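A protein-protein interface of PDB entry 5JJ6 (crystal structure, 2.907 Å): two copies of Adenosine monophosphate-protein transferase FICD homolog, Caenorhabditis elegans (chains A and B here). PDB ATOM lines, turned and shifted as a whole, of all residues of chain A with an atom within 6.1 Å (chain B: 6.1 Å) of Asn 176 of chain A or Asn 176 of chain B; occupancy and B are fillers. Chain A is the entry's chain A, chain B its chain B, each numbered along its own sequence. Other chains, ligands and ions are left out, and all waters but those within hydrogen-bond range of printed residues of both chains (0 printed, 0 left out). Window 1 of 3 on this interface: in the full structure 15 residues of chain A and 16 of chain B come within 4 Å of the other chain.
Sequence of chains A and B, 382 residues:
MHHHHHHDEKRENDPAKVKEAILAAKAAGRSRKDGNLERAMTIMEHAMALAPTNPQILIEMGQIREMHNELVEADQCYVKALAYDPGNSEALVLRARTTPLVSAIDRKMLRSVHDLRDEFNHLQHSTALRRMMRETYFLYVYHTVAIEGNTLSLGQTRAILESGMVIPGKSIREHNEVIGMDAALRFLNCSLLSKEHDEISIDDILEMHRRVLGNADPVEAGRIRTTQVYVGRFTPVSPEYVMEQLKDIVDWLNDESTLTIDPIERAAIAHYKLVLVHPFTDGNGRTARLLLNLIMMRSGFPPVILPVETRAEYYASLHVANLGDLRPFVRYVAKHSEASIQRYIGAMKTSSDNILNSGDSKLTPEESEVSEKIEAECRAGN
Ile 172 of chain A touches His 175 of chain B, and with the chains exchanged His 175 of chain A touches Ile 172 of chain B.
Asn 176 of chain A touches its own counterpart, Asn 176 of chain B.
Asn 215 of chain A touches its own counterpart, Asn 215 of chain B.
Asn 215 of chain A touches Ala 216 of chain B, but with the chains exchanged Ala 216 of chain A does not touch Asn 215 of chain B (4.6 Å).
Positions printed for both chains: 171, 172, 173, 174, 175, 176, 177, 178, 179, 180, 181, 212, 215 and 216.
Hydrophobic or aromatic side chains of chain A that line the printed part of chain B: Ile 172 and His 175.
Along chain A the printed residues that touch a printed residue of chain B span positions 172 to 215.
Of the 16 printed residues of chain B, 5 touch a printed residue of chain A.
Printed residues of chain B that touch a printed residue of chain A: Ile 172, His 175, Asn 176, Asn 215 and Ala 216.
Along chain B the printed residues that touch a printed residue of chain A span positions 172 to 216.
Among the printed residues, 5 pairs touch across the chains.
Among the printed residues, no Asp or Glu carboxylate lies within 4 Å of a Lys or Arg side-chain nitrogen of the other chain.
ND2 of Asn 176 of chain B lies within hydrogen-bond range of O of Asn 215 of chain B (3.3 Å).
The side-chain amide nitrogen of Asn 176 of chain A sits at hydrogen-bond distance from the backbone carbonyl oxygen of Asn 215 of chain A (3.3 Å).
O of Ser 171 of chain B sits at hydrogen-bond distance from ND1 of His 175 of chain B, at 2.8 Å.
O of Ser 171 of chain A is in hydrogen-bond range of ND1 of His 175 of chain A, 2.8 Å away.
The side-chain amide oxygen of Asn 176 of chain A is in hydrogen-bond range of the side-chain amide nitrogen of Asn 176 of chain B (3.0 Å).
The backbone carbonyl oxygen (O) of Asn 215 of chain B is in hydrogen-bond range of the side-chain amide nitrogen (ND2) of Asn 215 of chain A.
Of chain A, only Asn 176 comes within 4 Å of Asn 176 of chain B.
Printed residues of chain A within 4 Å of His 175 of chain B: Ile 172 (3.7 Å).
Of the printed residues of chain A, Ile 172 of chain B touches His 175 (3.9 Å).
Printed residues of chain A within 4 Å of Asn 215 of chain B: Asn 215.
Printed residues of chain B within 4 Å of His 175 of chain A: Ile 172.
Arg 173 of chain B touches none of the printed residues of chain A.
The nearest printed residue of chain A that does not touch Ala 216 of chain B is Ile 179 of chain A (6.3 Å).
Among the printed residues, pairs that only touch across the chains: Ile 172 of chain A with His 175 of chain B, His 175 of chain A with Ile 172 of chain B and Asn 215 of chain A with Ala 216 of chain B.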
ATOM      1  N   SER A 171      -1.872  17.060 -13.587  1.00  0.00           N
ATOM      2  CA  SER A 171      -2.450  16.042 -14.463  1.00  0.00           C
ATOM      3  C   SER A 171      -1.859  16.135 -15.866  1.00  0.00           C
ATOM      4  O   SER A 171      -1.534  17.237 -16.320  1.00  0.00           O
ATOM      5  CB  SER A 171      -3.974  16.163 -14.520  1.00  0.00           C
ATOM      6  OG  SER A 171      -4.380  17.196 -15.403  1.00  0.00           O
ATOM      7  N   ILE A 172      -1.717  14.997 -16.550  1.00  0.00           N
ATOM      8  CA  ILE A 172      -1.279  14.995 -17.950  1.00  0.00           C
ATOM      9  C   ILE A 172      -2.212  15.864 -18.813  1.00  0.00           C
ATOM     10  O   ILE A 172      -1.766  16.508 -19.765  1.00  0.00           O
ATOM     11  CB  ILE A 172      -1.206  13.557 -18.527  1.00  0.00           C
ATOM     12  CG1 ILE A 172      -0.320  13.507 -19.767  1.00  0.00           C
ATOM     13  CG2 ILE A 172      -2.578  13.032 -18.880  1.00  0.00           C
ATOM     14  CD1 ILE A 172       1.120  13.858 -19.486  1.00  0.00           C
ATOM     15  N   ARG A 173      -3.489  15.929 -18.448  1.00  0.00           N
ATOM     16  CA  ARG A 173      -4.474  16.712 -19.188  1.00  0.00           C
ATOM     17  C   ARG A 173      -4.119  18.217 -19.215  1.00  0.00           C
ATOM     18  O   ARG A 173      -4.283  18.879 -20.247  1.00  0.00           O
ATOM     19  CB  ARG A 173      -5.852  16.502 -18.560  1.00  0.00           C
ATOM     20  CG  ARG A 173      -7.011  17.255 -19.185  1.00  0.00           C
ATOM     21  CD  ARG A 173      -7.988  17.685 -18.072  1.00  0.00           C
ATOM     22  NE  ARG A 173      -7.788  16.917 -16.829  1.00  0.00           N
ATOM     23  CZ  ARG A 173      -7.595  17.456 -15.618  1.00  0.00           C
ATOM     24  NH1 ARG A 173      -7.573  18.782 -15.476  1.00  0.00           N
ATOM     25  NH2 ARG A 173      -7.415  16.671 -14.552  1.00  0.00           N
ATOM     26  N   GLU A 174      -3.615  18.746 -18.094  1.00  0.00           N
ATOM     27  CA  GLU A 174      -3.234  20.165 -18.009  1.00  0.00           C
ATOM     28  C   GLU A 174      -2.027  20.500 -18.899  1.00  0.00           C
ATOM     29  O   GLU A 174      -2.042  21.492 -19.676  1.00  0.00           O
ATOM     30  CB  GLU A 174      -2.949  20.550 -16.549  1.00  0.00           C
ATOM     31  CG  GLU A 174      -4.129  20.357 -15.592  1.00  0.00           C
ATOM     32  CD  GLU A 174      -3.836  20.814 -14.148  1.00  0.00           C
ATOM     33  OE1 GLU A 174      -3.072  20.115 -13.430  1.00  0.00           O
ATOM     34  OE2 GLU A 174      -4.361  21.877 -13.729  1.00  0.00           O
ATOM     35  N   HIS A 175      -1.001  19.659 -18.804  1.00  0.00           N
ATOM     36  CA  HIS A 175       0.151  19.744 -19.692  1.00  0.00           C
ATOM     37  C   HIS A 175      -0.333  19.788 -21.131  1.00  0.00           C
ATOM     38  O   HIS A 175       0.085  20.637 -21.929  1.00  0.00           O
ATOM     39  CB  HIS A 175       1.085  18.548 -19.543  1.00  0.00           C
ATOM     40  CG  HIS A 175       1.740  18.435 -18.200  1.00  0.00           C
ATOM     41  ND1 HIS A 175       1.076  17.975 -17.089  1.00  0.00           N
ATOM     42  CD2 HIS A 175       3.009  18.692 -17.807  1.00  0.00           C
ATOM     43  CE1 HIS A 175       1.908  17.947 -16.060  1.00  0.00           C
ATOM     44  NE2 HIS A 175       3.081  18.382 -16.469  1.00  0.00           N
ATOM     45  N   ASN A 176      -1.188  18.823 -21.464  1.00  0.00           N
ATOM     46  CA  ASN A 176      -1.696  18.691 -22.822  1.00  0.00           C
ATOM     47  C   ASN A 176      -2.493  19.877 -23.312  1.00  0.00           C
ATOM     48  O   ASN A 176      -2.436  20.198 -24.501  1.00  0.00           O
ATOM     49  CB  ASN A 176      -2.532  17.435 -22.946  1.00  0.00           C
ATOM     50  CG  ASN A 176      -1.681  16.220 -23.167  1.00  0.00           C
ATOM     51  OD1 ASN A 176      -0.503  16.336 -23.524  1.00  0.00           O
ATOM     52  ND2 ASN A 176      -2.258  15.041 -22.948  1.00  0.00           N
ATOM     53  N   GLU A 177      -3.218  20.539 -22.415  1.00  0.00           N
ATOM     54  CA  GLU A 177      -3.946  21.736 -22.811  1.00  0.00           C
ATOM     55  C   GLU A 177      -2.962  22.815 -23.206  1.00  0.00           C
ATOM     56  O   GLU A 177      -3.132  23.485 -24.241  1.00  0.00           O
ATOM     57  CB  GLU A 177      -4.856  22.226 -21.697  1.00  0.00           C
ATOM     58  CG  GLU A 177      -6.113  21.392 -21.565  1.00  0.00           C
ATOM     59  CD  GLU A 177      -6.959  21.791 -20.377  1.00  0.00           C
ATOM     60  OE1 GLU A 177      -6.674  22.854 -19.774  1.00  0.00           O
ATOM     61  OE2 GLU A 177      -7.900  21.032 -20.045  1.00  0.00           O
ATOM     62  N   VAL A 178      -1.916  22.967 -22.393  1.00  0.00           N
ATOM     63  CA  VAL A 178      -0.847  23.915 -22.738  1.00  0.00           C
ATOM     64  C   VAL A 178      -0.193  23.604 -24.109  1.00  0.00           C
ATOM     65  O   VAL A 178      -0.101  24.499 -24.978  1.00  0.00           O
ATOM     66  CB  VAL A 178       0.207  23.942 -21.640  1.00  0.00           C
ATOM     67  CG1 VAL A 178       1.458  24.648 -22.108  1.00  0.00           C
ATOM     68  CG2 VAL A 178      -0.369  24.613 -20.408  1.00  0.00           C
ATOM     69  N   ILE A 179       0.231  22.346 -24.303  1.00  0.00           N
ATOM     70  CA  ILE A 179       0.857  21.892 -25.561  1.00  0.00           C
ATOM     71  C   ILE A 179      -0.042  22.185 -26.776  1.00  0.00           C
ATOM     72  O   ILE A 179       0.405  22.724 -27.809  1.00  0.00           O
ATOM     73  CB  ILE A 179       1.128  20.357 -25.562  1.00  0.00           C
ATOM     74  CG1 ILE A 179       2.018  19.918 -24.404  1.00  0.00           C
ATOM     75  CG2 ILE A 179       1.699  19.901 -26.906  1.00  0.00           C
ATOM     76  CD1 ILE A 179       3.463  20.134 -24.639  1.00  0.00           C
ATOM     77  N   GLY A 180      -1.309  21.790 -26.645  1.00  0.00           N
ATOM     78  CA  GLY A 180      -2.308  22.035 -27.666  1.00  0.00           C
ATOM     79  C   GLY A 180      -2.390  23.505 -28.017  1.00  0.00           C
ATOM     80  O   GLY A 180      -2.374  23.872 -29.194  1.00  0.00           O
ATOM     81  N   MET A 181      -2.465  24.359 -26.997  1.00  0.00           N
ATOM     82  CA  MET A 181      -2.558  25.792 -27.253  1.00  0.00           C
ATOM     83  C   MET A 181      -1.339  26.319 -28.003  1.00  0.00           C
ATOM     84  O   MET A 181      -1.474  27.113 -28.934  1.00  0.00           O
ATOM     85  CB  MET A 181      -2.749  26.565 -25.964  1.00  0.00           C
ATOM     86  CG  MET A 181      -3.039  28.032 -26.206  1.00  0.00           C
ATOM     87  SD  MET A 181      -4.548  28.340 -27.168  1.00  0.00           S
ATOM     88  CE  MET A 181      -5.708  27.259 -26.307  1.00  0.00           C
ATOM     89  N   VAL A 212      -5.776  22.888 -30.951  1.00  0.00           N
ATOM     90  CA  VAL A 212      -6.135  23.281 -29.603  1.00  0.00           C
ATOM     91  C   VAL A 212      -6.319  22.040 -28.748  1.00  0.00           C
ATOM     92  O   VAL A 212      -5.665  21.887 -27.718  1.00  0.00           O
ATOM     93  CB  VAL A 212      -7.454  24.101 -29.555  1.00  0.00           C
ATOM     94  CG1 VAL A 212      -8.037  24.094 -28.140  1.00  0.00           C
ATOM     95  CG2 VAL A 212      -7.238  25.521 -30.011  1.00  0.00           C
ATOM     96  N   ASN A 215      -3.817  17.098 -28.412  1.00  0.00           N
ATOM     97  CA  ASN A 215      -3.113  16.323 -27.416  1.00  0.00           C
ATOM     98  C   ASN A 215      -4.018  15.888 -26.270  1.00  0.00           C
ATOM     99  O   ASN A 215      -3.916  14.758 -25.800  1.00  0.00           O
ATOM    100  CB  ASN A 215      -1.944  17.133 -26.874  1.00  0.00           C
ATOM    101  CG  ASN A 215      -1.031  17.629 -27.962  1.00  0.00           C
ATOM    102  OD1 ASN A 215      -1.230  18.709 -28.525  1.00  0.00           O
ATOM    103  ND2 ASN A 215      -0.002  16.849 -28.258  1.00  0.00           N
ATOM    104  N   ALA A 216      -4.899  16.780 -25.823  1.00  0.00           N
ATOM    105  CA  ALA A 216      -5.749  16.506 -24.661  1.00  0.00           C
ATOM    106  C   ALA A 216      -6.880  15.515 -24.975  1.00  0.00           C
ATOM    107  O   ALA A 216      -7.257  14.713 -24.129  1.00  0.00           O
ATOM    108  CB  ALA A 216      -6.320  17.795 -24.117  1.00  0.00           C
ATOM    109  N   ARG A 286     -11.653  28.230 -25.712  1.00  0.00           N
ATOM    110  CA  ARG A 286     -10.272  28.443 -26.132  1.00  0.00           C
ATOM    111  C   ARG A 286     -10.193  28.839 -27.614  1.00  0.00           C
ATOM    112  O   ARG A 286      -9.475  29.789 -27.978  1.00  0.00           O
ATOM    113  CB  ARG A 286      -9.430  27.195 -25.872  1.00  0.00           C
ATOM    114  CG  ARG A 286      -8.956  27.042 -24.449  1.00  0.00           C
ATOM    115  CD  ARG A 286      -8.299  25.693 -24.227  1.00  0.00           C
ATOM    116  NE  ARG A 286      -9.261  24.640 -23.918  1.00  0.00           N
ATOM    117  CZ  ARG A 286      -8.955  23.346 -23.875  1.00  0.00           C
ATOM    118  NH1 ARG A 286      -7.707  22.955 -24.114  1.00  0.00           N
ATOM    119  NH2 ARG A 286      -9.889  22.441 -23.591  1.00  0.00           N
ATOM    120  N   SER B 171       9.875  13.235 -19.850  1.00  0.00           N
ATOM    121  CA  SER B 171       9.249  13.756 -21.062  1.00  0.00           C
ATOM    122  C   SER B 171       7.732  13.583 -21.163  1.00  0.00           C
ATOM    123  O   SER B 171       7.199  12.475 -21.019  1.00  0.00           O
ATOM    124  CB  SER B 171       9.913  13.059 -22.249  1.00  0.00           C
ATOM    125  OG  SER B 171       9.123  13.109 -23.419  1.00  0.00           O
ATOM    126  N   ILE B 172       7.051  14.685 -21.470  1.00  0.00           N
ATOM    127  CA  ILE B 172       5.606  14.682 -21.719  1.00  0.00           C
ATOM    128  C   ILE B 172       5.246  13.834 -22.938  1.00  0.00           C
ATOM    129  O   ILE B 172       4.207  13.139 -22.973  1.00  0.00           O
ATOM    130  CB  ILE B 172       5.092  16.123 -21.920  1.00  0.00           C
ATOM    131  CG1 ILE B 172       5.455  16.974 -20.703  1.00  0.00           C
ATOM    132  CG2 ILE B 172       3.607  16.143 -22.167  1.00  0.00           C
ATOM    133  CD1 ILE B 172       5.329  18.473 -20.929  1.00  0.00           C
ATOM    134  N   ARG B 173       6.099  13.890 -23.937  1.00  0.00           N
ATOM    135  CA  ARG B 173       5.912  13.156 -25.153  1.00  0.00           C
ATOM    136  C   ARG B 173       5.901  11.687 -24.891  1.00  0.00           C
ATOM    137  O   ARG B 173       5.138  10.993 -25.466  1.00  0.00           O
ATOM    138  CB  ARG B 173       7.019  13.514 -26.116  1.00  0.00           C
ATOM    139  CG  ARG B 173       6.866  13.012 -27.528  1.00  0.00           C
ATOM    140  CD  ARG B 173       8.197  13.055 -28.226  1.00  0.00           C
ATOM    141  NE  ARG B 173       9.052  11.947 -27.832  1.00  0.00           N
ATOM    142  CZ  ARG B 173      10.139  12.046 -27.090  1.00  0.00           C
ATOM    143  NH1 ARG B 173      10.548  13.205 -26.637  1.00  0.00           N
ATOM    144  NH2 ARG B 173      10.819  10.970 -26.806  1.00  0.00           N
ATOM    145  N   GLU B 174       6.752  11.203 -24.023  1.00  0.00           N
ATOM    146  CA  GLU B 174       6.782   9.776 -23.693  1.00  0.00           C
ATOM    147  C   GLU B 174       5.482   9.326 -22.997  1.00  0.00           C
ATOM    148  O   GLU B 174       4.946   8.236 -23.295  1.00  0.00           O
ATOM    149  CB  GLU B 174       7.989   9.442 -22.817  1.00  0.00           C
ATOM    150  CG  GLU B 174       9.330   9.798 -23.424  1.00  0.00           C
ATOM    151  CD  GLU B 174      10.498   9.350 -22.555  1.00  0.00           C
ATOM    152  OE1 GLU B 174      10.689   9.954 -21.456  1.00  0.00           O
ATOM    153  OE2 GLU B 174      11.237   8.420 -22.981  1.00  0.00           O
ATOM    154  N   HIS B 175       5.002  10.132 -22.046  1.00  0.00           N
ATOM    155  CA  HIS B 175       3.684   9.896 -21.466  1.00  0.00           C
ATOM    156  C   HIS B 175       2.628   9.745 -22.558  1.00  0.00           C
ATOM    157  O   HIS B 175       1.916   8.729 -22.628  1.00  0.00           O
ATOM    158  CB  HIS B 175       3.281  11.032 -20.521  1.00  0.00           C
ATOM    159  CG  HIS B 175       4.068  11.072 -19.255  1.00  0.00           C
ATOM    160  ND1 HIS B 175       5.376  11.514 -19.198  1.00  0.00           N
ATOM    161  CD2 HIS B 175       3.739  10.721 -17.991  1.00  0.00           C
ATOM    162  CE1 HIS B 175       5.814  11.432 -17.957  1.00  0.00           C
ATOM    163  NE2 HIS B 175       4.839  10.952 -17.202  1.00  0.00           N
ATOM    164  N   ASN B 176       2.557  10.743 -23.432  1.00  0.00           N
ATOM    165  CA  ASN B 176       1.556  10.729 -24.488  1.00  0.00           C
ATOM    166  C   ASN B 176       1.658   9.518 -25.423  1.00  0.00           C
ATOM    167  O   ASN B 176       0.631   9.042 -25.930  1.00  0.00           O
ATOM    168  CB  ASN B 176       1.642  12.005 -25.307  1.00  0.00           C
ATOM    169  CG  ASN B 176       0.884  13.138 -24.678  1.00  0.00           C
ATOM    170  OD1 ASN B 176       0.041  12.920 -23.796  1.00  0.00           O
ATOM    171  ND2 ASN B 176       1.166  14.360 -25.126  1.00  0.00           N
ATOM    172  N   GLU B 177       2.880   9.031 -25.650  1.00  0.00           N
ATOM    173  CA  GLU B 177       3.103   7.816 -26.428  1.00  0.00           C
ATOM    174  C   GLU B 177       2.549   6.593 -25.719  1.00  0.00           C
ATOM    175  O   GLU B 177       1.870   5.766 -26.331  1.00  0.00           O
ATOM    176  CB  GLU B 177       4.590   7.635 -26.709  1.00  0.00           C
ATOM    177  CG  GLU B 177       5.092   8.488 -27.866  1.00  0.00           C
ATOM    178  CD  GLU B 177       6.618   8.492 -28.003  1.00  0.00           C
ATOM    179  OE1 GLU B 177       7.309   7.714 -27.290  1.00  0.00           O
ATOM    180  OE2 GLU B 177       7.125   9.274 -28.845  1.00  0.00           O
ATOM    181  N   VAL B 178       2.816   6.491 -24.422  1.00  0.00           N
ATOM    182  CA  VAL B 178       2.281   5.387 -23.639  1.00  0.00           C
ATOM    183  C   VAL B 178       0.753   5.374 -23.716  1.00  0.00           C
ATOM    184  O   VAL B 178       0.134   4.357 -24.085  1.00  0.00           O
ATOM    185  CB  VAL B 178       2.758   5.481 -22.172  1.00  0.00           C
ATOM    186  CG1 VAL B 178       1.981   4.552 -21.272  1.00  0.00           C
ATOM    187  CG2 VAL B 178       4.237   5.156 -22.095  1.00  0.00           C
ATOM    188  N   ILE B 179       0.154   6.520 -23.399  1.00  0.00           N
ATOM    189  CA  ILE B 179      -1.301   6.657 -23.412  1.00  0.00           C
ATOM    190  C   ILE B 179      -1.917   6.337 -24.776  1.00  0.00           C
ATOM    191  O   ILE B 179      -2.875   5.556 -24.870  1.00  0.00           O
ATOM    192  CB  ILE B 179      -1.715   8.069 -22.941  1.00  0.00           C
ATOM    193  CG1 ILE B 179      -1.418   8.207 -21.438  1.00  0.00           C
ATOM    194  CG2 ILE B 179      -3.193   8.287 -23.150  1.00  0.00           C
ATOM    195  CD1 ILE B 179      -0.966   9.589 -21.001  1.00  0.00           C
ATOM    196  N   GLY B 180      -1.360   6.939 -25.821  1.00  0.00           N
ATOM    197  CA  GLY B 180      -1.779   6.662 -27.187  1.00  0.00           C
ATOM    198  C   GLY B 180      -1.722   5.191 -27.563  1.00  0.00           C
ATOM    199  O   GLY B 180      -2.680   4.664 -28.128  1.00  0.00           O
ATOM    200  N   MET B 181      -0.609   4.521 -27.263  1.00  0.00           N
ATOM    201  CA  MET B 181      -0.499   3.106 -27.590  1.00  0.00           C
ATOM    202  C   MET B 181      -1.571   2.297 -26.886  1.00  0.00           C
ATOM    203  O   MET B 181      -2.222   1.454 -27.500  1.00  0.00           O
ATOM    204  CB  MET B 181       0.867   2.539 -27.218  1.00  0.00           C
ATOM    205  CG  MET B 181       1.753   2.163 -28.407  1.00  0.00           C
ATOM    206  SD  MET B 181       1.064   1.049 -29.677  1.00  0.00           S
ATOM    207  CE  MET B 181       0.281  -0.184 -28.655  1.00  0.00           C
ATOM    208  N   ARG B 211      -4.973   6.476 -33.110  1.00  0.00           N
ATOM    209  CA  ARG B 211      -4.849   6.303 -31.669  1.00  0.00           C
ATOM    210  C   ARG B 211      -3.386   6.165 -31.183  1.00  0.00           C
ATOM    211  O   ARG B 211      -3.043   6.632 -30.090  1.00  0.00           O
ATOM    212  CB  ARG B 211      -5.706   5.126 -31.231  1.00  0.00           C
ATOM    213  CG  ARG B 211      -7.168   5.525 -31.249  1.00  0.00           C
ATOM    214  CD  ARG B 211      -8.126   4.373 -31.093  1.00  0.00           C
ATOM    215  NE  ARG B 211      -9.490   4.857 -30.888  1.00  0.00           N
ATOM    216  CZ  ARG B 211     -10.268   5.330 -31.857  1.00  0.00           C
ATOM    217  NH1 ARG B 211      -9.816   5.371 -33.107  1.00  0.00           N
ATOM    218  NH2 ARG B 211     -11.497   5.757 -31.582  1.00  0.00           N
ATOM    219  N   VAL B 212      -2.530   5.535 -31.985  1.00  0.00           N
ATOM    220  CA  VAL B 212      -1.104   5.409 -31.666  1.00  0.00           C
ATOM    221  C   VAL B 212      -0.477   6.783 -31.474  1.00  0.00           C
ATOM    222  O   VAL B 212       0.262   7.007 -30.516  1.00  0.00           O
ATOM    223  CB  VAL B 212      -0.323   4.640 -32.761  1.00  0.00           C
ATOM    224  CG1 VAL B 212       1.164   4.908 -32.652  1.00  0.00           C
ATOM    225  CG2 VAL B 212      -0.572   3.158 -32.650  1.00  0.00           C
ATOM    226  N   ASN B 215      -2.346  11.402 -29.032  1.00  0.00           N
ATOM    227  CA  ASN B 215      -1.885  12.291 -27.983  1.00  0.00           C
ATOM    228  C   ASN B 215      -0.502  12.876 -28.251  1.00  0.00           C
ATOM    229  O   ASN B 215      -0.276  14.060 -28.036  1.00  0.00           O
ATOM    230  CB  ASN B 215      -1.895  11.568 -26.644  1.00  0.00           C
ATOM    231  CG  ASN B 215      -3.248  10.980 -26.315  1.00  0.00           C
ATOM    232  OD1 ASN B 215      -3.545   9.837 -26.643  1.00  0.00           O
ATOM    233  ND2 ASN B 215      -4.088  11.778 -25.677  1.00  0.00           N
ATOM    234  N   ALA B 216       0.423  12.060 -28.740  1.00  0.00           N
ATOM    235  CA  ALA B 216       1.805  12.508 -28.880  1.00  0.00           C
ATOM    236  C   ALA B 216       1.978  13.487 -30.032  1.00  0.00           C
ATOM    237  O   ALA B 216       2.725  14.453 -29.920  1.00  0.00           O
ATOM    238  CB  ALA B 216       2.725  11.313 -29.066  1.00  0.00           C
ATOM    239  N   ASP B 217       1.261  13.257 -31.125  1.00  0.00           N
ATOM    240  CA  ASP B 217       1.400  14.074 -32.325  1.00  0.00           C
ATOM    241  C   ASP B 217       0.076  14.128 -33.078  1.00  0.00           C
ATOM    242  O   ASP B 217      -0.100  13.443 -34.079  1.00  0.00           O
ATOM    243  CB  ASP B 217       2.501  13.505 -33.224  1.00  0.00           C
ATOM    244  CG  ASP B 217       3.021  14.514 -34.240  1.00  0.00           C
ATOM    245  OD1 ASP B 217       2.409  15.597 -34.379  1.00  0.00           O
ATOM    246  OD2 ASP B 217       4.041  14.214 -34.905  1.00  0.00           O
